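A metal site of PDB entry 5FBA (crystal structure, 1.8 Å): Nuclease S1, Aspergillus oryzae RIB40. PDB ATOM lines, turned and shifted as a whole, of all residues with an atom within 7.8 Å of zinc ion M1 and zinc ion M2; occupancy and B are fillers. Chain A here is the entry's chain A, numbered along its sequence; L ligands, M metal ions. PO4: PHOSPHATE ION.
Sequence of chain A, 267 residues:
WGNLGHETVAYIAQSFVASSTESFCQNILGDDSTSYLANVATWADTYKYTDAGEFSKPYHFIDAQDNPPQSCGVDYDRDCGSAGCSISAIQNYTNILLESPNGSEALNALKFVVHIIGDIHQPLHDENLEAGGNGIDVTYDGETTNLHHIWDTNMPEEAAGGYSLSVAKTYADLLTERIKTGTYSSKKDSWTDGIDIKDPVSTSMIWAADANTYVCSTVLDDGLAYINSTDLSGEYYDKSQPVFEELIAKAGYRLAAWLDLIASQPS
Zinc ion M2 is bound by O1 of the ligand (2.0 Å), NE2 of His 6 (2.1 Å), N of Trp 1 (2.1 Å), OD1 of Asp 119 (2.1 Å) and O of Trp 1 (2.2 Å).
A ring nitrogen (ND1) of His 125 lies within hydrogen-bond range of the backbone carbonyl oxygen of His 60.
The backbone carbonyl oxygen (O) of His 115 sits close to a ring nitrogen (ND1) of His 6 (3.5 Å).
A ring nitrogen (ND1) of His 115 sits at hydrogen-bond distance from the backbone carbonyl oxygen (O) of Ala 41 (2.7 Å).
N of Trp 1 sits close to OD1 of Asp 152 (2.9 Å).
The backbone carbonyl oxygen (O) of Gly 118 sits at hydrogen-bond distance from the indole nitrogen (NE1) of Trp 1 (2.8 Å).
The side-chain carboxylate (OD1) of Asp 45 sits close to the side-chain amino group (NZ) of Lys 48, 2.9 Å away.
Zinc ion M1 is bound by O1 of the ligand, OD2 of Asp 119, ND1 of His 60, NE2 of His 115 and OD1 of Asp 45.
Of the 26 residues printed, 5 come within 4 Å of zinc ion M2.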
ATOM      1  N   TRP A   1      13.385  32.958  10.377  1.00  0.00           N
ATOM      2  CA  TRP A   1      12.970  33.648  11.621  1.00  0.00           C
ATOM      3  C   TRP A   1      13.699  32.971  12.774  1.00  0.00           C
ATOM      4  O   TRP A   1      14.155  31.804  12.681  1.00  0.00           O
ATOM      5  CB  TRP A   1      11.456  33.561  11.879  1.00  0.00           C
ATOM      6  CG  TRP A   1      10.559  34.027  10.767  1.00  0.00           C
ATOM      7  CD1 TRP A   1       9.882  33.240   9.888  1.00  0.00           C
ATOM      8  CD2 TRP A   1      10.266  35.406  10.394  1.00  0.00           C
ATOM      9  NE1 TRP A   1       9.141  34.023   9.022  1.00  0.00           N
ATOM     10  CE2 TRP A   1       9.392  35.349   9.273  1.00  0.00           C
ATOM     11  CE3 TRP A   1      10.675  36.652  10.877  1.00  0.00           C
ATOM     12  CZ2 TRP A   1       8.906  36.479   8.643  1.00  0.00           C
ATOM     13  CZ3 TRP A   1      10.180  37.827  10.228  1.00  0.00           C
ATOM     14  CH2 TRP A   1       9.295  37.720   9.112  1.00  0.00           C
ATOM     15  N   GLY A   2      13.782  33.695  13.864  1.00  0.00           N
ATOM     16  CA  GLY A   2      14.202  33.096  15.154  1.00  0.00           C
ATOM     17  C   GLY A   2      13.022  32.367  15.752  1.00  0.00           C
ATOM     18  O   GLY A   2      11.985  32.222  15.091  1.00  0.00           O
ATOM     19  N   ASN A   3      13.162  31.932  17.000  1.00  0.00           N
ATOM     20  CA  ASN A   3      12.196  31.028  17.627  1.00  0.00           C
ATOM     21  C   ASN A   3      10.823  31.643  17.744  1.00  0.00           C
ATOM     22  O   ASN A   3       9.843  31.006  17.469  1.00  0.00           O
ATOM     23  CB  ASN A   3      12.702  30.587  19.002  1.00  0.00           C
ATOM     24  CG  ASN A   3      13.976  29.751  18.885  1.00  0.00           C
ATOM     25  OD1 ASN A   3      14.347  29.230  17.820  1.00  0.00           O
ATOM     26  ND2 ASN A   3      14.673  29.663  19.962  1.00  0.00           N
ATOM     27  N   GLY A   5       9.318  34.080  15.955  1.00  0.00           N
ATOM     28  CA  GLY A   5       8.730  34.043  14.626  1.00  0.00           C
ATOM     29  C   GLY A   5       8.149  32.668  14.251  1.00  0.00           C
ATOM     30  O   GLY A   5       7.020  32.574  13.837  1.00  0.00           O
ATOM     31  N   HIS A   6       8.944  31.625  14.377  1.00  0.00           N
ATOM     32  CA  HIS A   6       8.466  30.267  14.066  1.00  0.00           C
ATOM     33  C   HIS A   6       7.326  29.787  14.911  1.00  0.00           C
ATOM     34  O   HIS A   6       6.390  29.144  14.402  1.00  0.00           O
ATOM     35  CB  HIS A   6       9.619  29.319  14.150  1.00  0.00           C
ATOM     36  CG  HIS A   6      10.490  29.410  12.963  1.00  0.00           C
ATOM     37  ND1 HIS A   6      10.029  29.164  11.691  1.00  0.00           N
ATOM     38  CD2 HIS A   6      11.765  29.823  12.830  1.00  0.00           C
ATOM     39  CE1 HIS A   6      11.013  29.328  10.831  1.00  0.00           C
ATOM     40  NE2 HIS A   6      12.078  29.746  11.484  1.00  0.00           N
ATOM     41  N   ALA A  41       8.156  23.865  16.118  1.00  0.00           N
ATOM     42  CA  ALA A  41       8.364  24.843  15.079  1.00  0.00           C
ATOM     43  C   ALA A  41       9.836  25.309  14.970  1.00  0.00           C
ATOM     44  O   ALA A  41      10.182  25.890  13.937  1.00  0.00           O
ATOM     45  CB  ALA A  41       7.421  26.043  15.279  1.00  0.00           C
ATOM     46  N   THR A  42      10.652  25.101  16.001  1.00  0.00           N
ATOM     47  CA  THR A  42      12.079  25.547  15.980  1.00  0.00           C
ATOM     48  C   THR A  42      13.038  24.392  15.805  1.00  0.00           C
ATOM     49  O   THR A  42      14.254  24.603  15.702  1.00  0.00           O
ATOM     50  CB  THR A  42      12.472  26.303  17.259  1.00  0.00           C
ATOM     51  OG1 THR A  42      12.426  25.361  18.323  1.00  0.00           O
ATOM     52  CG2 THR A  42      11.455  27.378  17.585  1.00  0.00           C
ATOM     53  N   ALA A  44      13.912  22.422  13.454  1.00  0.00           N
ATOM     54  CA  ALA A  44      14.835  22.394  12.326  1.00  0.00           C
ATOM     55  C   ALA A  44      16.074  23.295  12.537  1.00  0.00           C
ATOM     56  O   ALA A  44      17.163  22.968  12.026  1.00  0.00           O
ATOM     57  CB  ALA A  44      14.113  22.697  11.023  1.00  0.00           C
ATOM     58  N   ASP A  45      15.930  24.346  13.316  1.00  0.00           N
ATOM     59  CA  ASP A  45      17.006  25.268  13.643  1.00  0.00           C
ATOM     60  C   ASP A  45      18.025  24.650  14.654  1.00  0.00           C
ATOM     61  O   ASP A  45      19.202  24.919  14.539  1.00  0.00           O
ATOM     62  CB  ASP A  45      16.501  26.635  14.158  1.00  0.00           C
ATOM     63  CG  ASP A  45      16.160  27.610  13.008  1.00  0.00           C
ATOM     64  OD1 ASP A  45      16.463  27.326  11.804  1.00  0.00           O
ATOM     65  OD2 ASP A  45      15.562  28.684  13.328  1.00  0.00           O
ATOM     66  N   THR A  46      17.570  23.755  15.508  1.00  0.00           N
ATOM     67  CA  THR A  46      18.458  22.851  16.254  1.00  0.00           C
ATOM     68  C   THR A  46      19.173  21.823  15.394  1.00  0.00           C
ATOM     69  O   THR A  46      20.384  21.639  15.455  1.00  0.00           O
ATOM     70  CB  THR A  46      17.627  22.186  17.364  1.00  0.00           C
ATOM     71  OG1 THR A  46      17.359  23.179  18.336  1.00  0.00           O
ATOM     72  CG2 THR A  46      18.342  21.002  18.021  1.00  0.00           C
ATOM     73  N   LYS A  48      19.869  21.539  12.275  1.00  0.00           N
ATOM     74  CA  LYS A  48      20.899  21.957  11.336  1.00  0.00           C
ATOM     75  C   LYS A  48      22.285  22.206  11.962  1.00  0.00           C
ATOM     76  O   LYS A  48      23.258  22.267  11.235  1.00  0.00           O
ATOM     77  CB  LYS A  48      20.411  23.205  10.550  1.00  0.00           C
ATOM     78  CG  LYS A  48      20.552  24.489  11.313  1.00  0.00           C
ATOM     79  CD  LYS A  48      19.854  25.607  10.608  1.00  0.00           C
ATOM     80  CE  LYS A  48      19.992  26.929  11.324  1.00  0.00           C
ATOM     81  NZ  LYS A  48      19.062  27.888  10.706  1.00  0.00           N
ATOM     82  N   SER A  56      20.863  19.609   6.229  1.00  0.00           N
ATOM     83  CA  SER A  56      19.652  20.396   6.172  1.00  0.00           C
ATOM     84  C   SER A  56      19.817  21.918   6.296  1.00  0.00           C
ATOM     85  O   SER A  56      18.821  22.606   6.181  1.00  0.00           O
ATOM     86  CB  SER A  56      18.654  19.888   7.259  1.00  0.00           C
ATOM     87  OG  SER A  56      19.134  20.081   8.589  1.00  0.00           O
ATOM     88  N   LYS A  57      21.022  22.451   6.530  1.00  0.00           N
ATOM     89  CA  LYS A  57      21.202  23.912   6.642  1.00  0.00           C
ATOM     90  C   LYS A  57      20.643  24.722   5.418  1.00  0.00           C
ATOM     91  O   LYS A  57      19.981  25.715   5.604  1.00  0.00           O
ATOM     92  CB  LYS A  57      22.673  24.293   6.790  1.00  0.00           C
ATOM     93  CG  LYS A  57      23.272  24.104   8.174  1.00  0.00           C
ATOM     94  CD  LYS A  57      24.709  24.595   8.124  1.00  0.00           C
ATOM     95  CE  LYS A  57      25.613  23.889   9.140  1.00  0.00           C
ATOM     96  NZ  LYS A  57      25.756  24.679  10.399  1.00  0.00           N
ATOM     97  N   TYR A  59      18.220  24.040   3.541  1.00  0.00           N
ATOM     98  CA  TYR A  59      16.754  23.915   3.451  1.00  0.00           C
ATOM     99  C   TYR A  59      16.011  25.073   4.044  1.00  0.00           C
ATOM    100  O   TYR A  59      14.786  25.171   3.900  1.00  0.00           O
ATOM    101  CB  TYR A  59      16.223  22.596   4.024  1.00  0.00           C
ATOM    102  CG  TYR A  59      16.830  21.275   3.466  1.00  0.00           C
ATOM    103  CD1 TYR A  59      17.725  21.252   2.390  1.00  0.00           C
ATOM    104  CD2 TYR A  59      16.436  20.047   4.011  1.00  0.00           C
ATOM    105  CE1 TYR A  59      18.245  20.040   1.915  1.00  0.00           C
ATOM    106  CE2 TYR A  59      16.900  18.866   3.516  1.00  0.00           C
ATOM    107  CZ  TYR A  59      17.812  18.866   2.471  1.00  0.00           C
ATOM    108  OH  TYR A  59      18.328  17.676   2.050  1.00  0.00           O
ATOM    109  N   HIS A  60      16.733  26.018   4.682  1.00  0.00           N
ATOM    110  CA  HIS A  60      16.068  27.143   5.294  1.00  0.00           C
ATOM    111  C   HIS A  60      15.869  28.327   4.372  1.00  0.00           C
ATOM    112  O   HIS A  60      15.174  29.267   4.772  1.00  0.00           O
ATOM    113  CB  HIS A  60      16.838  27.557   6.556  1.00  0.00           C
ATOM    114  CG  HIS A  60      16.844  26.462   7.579  1.00  0.00           C
ATOM    115  ND1 HIS A  60      16.198  26.584   8.790  1.00  0.00           N
ATOM    116  CD2 HIS A  60      17.249  25.170   7.484  1.00  0.00           C
ATOM    117  CE1 HIS A  60      16.266  25.424   9.428  1.00  0.00           C
ATOM    118  NE2 HIS A  60      16.910  24.564   8.657  1.00  0.00           N
ATOM    119  N   PHE A  61      16.490  28.275   3.193  1.00  0.00           N
ATOM    120  CA  PHE A  61      16.463  29.418   2.319  1.00  0.00           C
ATOM    121  C   PHE A  61      16.511  29.051   0.838  1.00  0.00           C
ATOM    122  O   PHE A  61      16.750  27.911   0.450  1.00  0.00           O
ATOM    123  CB  PHE A  61      17.605  30.388   2.680  1.00  0.00           C
ATOM    124  CG  PHE A  61      18.969  29.759   2.715  1.00  0.00           C
ATOM    125  CD1 PHE A  61      19.738  29.650   1.581  1.00  0.00           C
ATOM    126  CD2 PHE A  61      19.480  29.276   3.914  1.00  0.00           C
ATOM    127  CE1 PHE A  61      20.977  29.068   1.613  1.00  0.00           C
ATOM    128  CE2 PHE A  61      20.740  28.678   3.966  1.00  0.00           C
ATOM    129  CZ  PHE A  61      21.496  28.584   2.808  1.00  0.00           C
ATOM    130  N   HIS A 115       8.392  24.448   9.986  1.00  0.00           N
ATOM    131  CA  HIS A 115       9.489  25.399  10.122  1.00  0.00           C
ATOM    132  C   HIS A 115       9.705  26.160   8.796  1.00  0.00           C
ATOM    133  O   HIS A 115       9.719  27.383   8.744  1.00  0.00           O
ATOM    134  CB  HIS A 115      10.790  24.702  10.546  1.00  0.00           C
ATOM    135  CG  HIS A 115      11.901  25.654  10.791  1.00  0.00           C
ATOM    136  ND1 HIS A 115      12.062  26.306  12.008  1.00  0.00           N
ATOM    137  CD2 HIS A 115      12.907  26.091   9.996  1.00  0.00           C
ATOM    138  CE1 HIS A 115      13.098  27.118  11.935  1.00  0.00           C
ATOM    139  NE2 HIS A 115      13.622  27.021  10.727  1.00  0.00           N
ATOM    140  N   ILE A 116       9.798  25.391   7.717  1.00  0.00           N
ATOM    141  CA  ILE A 116      10.256  25.953   6.411  1.00  0.00           C
ATOM    142  C   ILE A 116       9.226  26.839   5.760  1.00  0.00           C
ATOM    143  O   ILE A 116       9.595  27.882   5.242  1.00  0.00           O
ATOM    144  CB  ILE A 116      10.784  24.889   5.481  1.00  0.00           C
ATOM    145  CG1 ILE A 116      12.073  24.337   6.084  1.00  0.00           C
ATOM    146  CG2 ILE A 116      11.118  25.451   4.091  1.00  0.00           C
ATOM    147  CD1 ILE A 116      12.481  22.971   5.517  1.00  0.00           C
ATOM    148  N   GLY A 118       7.444  28.723   7.430  1.00  0.00           N
ATOM    149  CA  GLY A 118       7.884  29.964   8.162  1.00  0.00           C
ATOM    150  C   GLY A 118       9.029  30.719   7.496  1.00  0.00           C
ATOM    151  O   GLY A 118       8.890  31.900   7.144  1.00  0.00           O
ATOM    152  N   ASP A 119      10.142  30.024   7.325  1.00  0.00           N
ATOM    153  CA  ASP A 119      11.326  30.603   6.701  1.00  0.00           C
ATOM    154  C   ASP A 119      11.120  31.257   5.297  1.00  0.00           C
ATOM    155  O   ASP A 119      11.685  32.320   4.992  1.00  0.00           O
ATOM    156  CB  ASP A 119      12.418  29.549   6.618  1.00  0.00           C
ATOM    157  CG  ASP A 119      13.232  29.465   7.889  1.00  0.00           C
ATOM    158  OD1 ASP A 119      13.073  30.409   8.709  1.00  0.00           O
ATOM    159  OD2 ASP A 119      14.059  28.529   8.023  1.00  0.00           O
ATOM    160  N   ILE A 120      10.297  30.618   4.496  1.00  0.00           N
ATOM    161  CA  ILE A 120       9.998  31.080   3.143  1.00  0.00           C
ATOM    162  C   ILE A 120       9.396  32.478   3.184  1.00  0.00           C
ATOM    163  O   ILE A 120       9.543  33.245   2.233  1.00  0.00           O
ATOM    164  CB  ILE A 120       9.105  30.048   2.426  1.00  0.00           C
ATOM    165  CG1 ILE A 120       9.954  28.859   1.989  1.00  0.00           C
ATOM    166  CG2 ILE A 120       8.421  30.668   1.213  1.00  0.00           C
ATOM    167  CD1 ILE A 120       9.121  27.654   1.581  1.00  0.00           C
ATOM    168  N   GLN A 122      10.228  34.817   5.463  1.00  0.00           N
ATOM    169  CA  GLN A 122      11.195  35.822   5.984  1.00  0.00           C
ATOM    170  C   GLN A 122      11.899  36.279   4.695  1.00  0.00           C
ATOM    171  O   GLN A 122      12.621  35.480   4.106  1.00  0.00           O
ATOM    172  CB  GLN A 122      12.156  35.171   6.995  1.00  0.00           C
ATOM    173  CG  GLN A 122      12.787  36.094   8.012  1.00  0.00           C
ATOM    174  CD  GLN A 122      13.834  37.035   7.408  1.00  0.00           C
ATOM    175  OE1 GLN A 122      13.552  37.789   6.486  1.00  0.00           O
ATOM    176  NE2 GLN A 122      15.033  36.997   7.939  1.00  0.00           N
ATOM    177  N   HIS A 125      15.386  35.159   3.869  1.00  0.00           N
ATOM    178  CA  HIS A 125      15.586  33.778   3.549  1.00  0.00           C
ATOM    179  C   HIS A 125      15.299  33.499   2.036  1.00  0.00           C
ATOM    180  O   HIS A 125      15.372  32.338   1.594  1.00  0.00           O
ATOM    181  CB  HIS A 125      14.699  32.951   4.442  1.00  0.00           C
ATOM    182  CG  HIS A 125      15.258  32.729   5.817  1.00  0.00           C
ATOM    183  ND1 HIS A 125      15.582  31.477   6.261  1.00  0.00           N
ATOM    184  CD2 HIS A 125      15.564  33.585   6.807  1.00  0.00           C
ATOM    185  CE1 HIS A 125      16.050  31.566   7.492  1.00  0.00           C
ATOM    186  NE2 HIS A 125      16.054  32.836   7.839  1.00  0.00           N
ATOM    187  N   HIS A 148      20.225  40.431   8.639  1.00  0.00           N
ATOM    188  CA  HIS A 148      19.454  39.195   8.723  1.00  0.00           C
ATOM    189  C   HIS A 148      18.889  38.915  10.130  1.00  0.00           C
ATOM    190  O   HIS A 148      17.708  38.559  10.285  1.00  0.00           O
ATOM    191  CB  HIS A 148      20.296  38.030   8.273  1.00  0.00           C
ATOM    192  CG  HIS A 148      19.502  36.783   8.147  1.00  0.00           C
ATOM    193  ND1 HIS A 148      19.152  36.247   6.931  1.00  0.00           N
ATOM    194  CD2 HIS A 148      18.969  35.993   9.102  1.00  0.00           C
ATOM    195  CE1 HIS A 148      18.449  35.153   7.153  1.00  0.00           C
ATOM    196  NE2 HIS A 148      18.275  35.016   8.453  1.00  0.00           N
ATOM    197  N   ASP A 152      15.097  38.225  11.431  1.00  0.00           N
ATOM    198  CA  ASP A 152      14.827  37.003  12.143  1.00  0.00           C
ATOM    199  C   ASP A 152      14.248  37.177  13.538  1.00  0.00           C
ATOM    200  O   ASP A 152      13.309  36.467  13.908  1.00  0.00           O
ATOM    201  CB  ASP A 152      16.064  36.112  12.253  1.00  0.00           C
ATOM    202  CG  ASP A 152      16.198  35.161  11.074  1.00  0.00           C
ATOM    203  OD1 ASP A 152      15.335  35.116  10.181  1.00  0.00           O
ATOM    204  OD2 ASP A 152      17.246  34.510  11.053  1.00  0.00           O
ATOM    205  N   THR A 153      14.826  38.121  14.288  1.00  0.00           N
ATOM    206  CA  THR A 153      14.750  38.109  15.740  1.00  0.00           C
ATOM    207  C   THR A 153      14.506  39.445  16.421  1.00  0.00           C
ATOM    208  O   THR A 153      13.480  39.607  17.079  1.00  0.00           O
ATOM    209  CB  THR A 153      16.040  37.478  16.266  1.00  0.00           C
ATOM    210  OG1 THR A 153      16.032  36.128  15.856  1.00  0.00           O
ATOM    211  CG2 THR A 153      16.148  37.523  17.842  1.00  0.00           C
HETATM  212  P   PO4 L   1      16.611  30.417  10.709  1.00  0.00           P
HETATM  213  O1  PO4 L   1      15.258  29.744  10.567  1.00  0.00           O
HETATM  214  O2  PO4 L   1      17.115  30.287  12.124  1.00  0.00           O
HETATM  215  O3  PO4 L   1      16.450  31.890  10.404  1.00  0.00           O
HETATM  216  O4  PO4 L   1      17.590  29.734   9.789  1.00  0.00           O
HETATM  217 ZN    ZN M   1      15.132  28.083   9.729  1.00  0.00          ZN
HETATM  218 ZN    ZN M   2      13.664  30.883  10.707  1.00  0.00          ZN
HETATM  219 ZN    ZN M   3      17.269  33.442   9.383  1.00  0.00          ZN
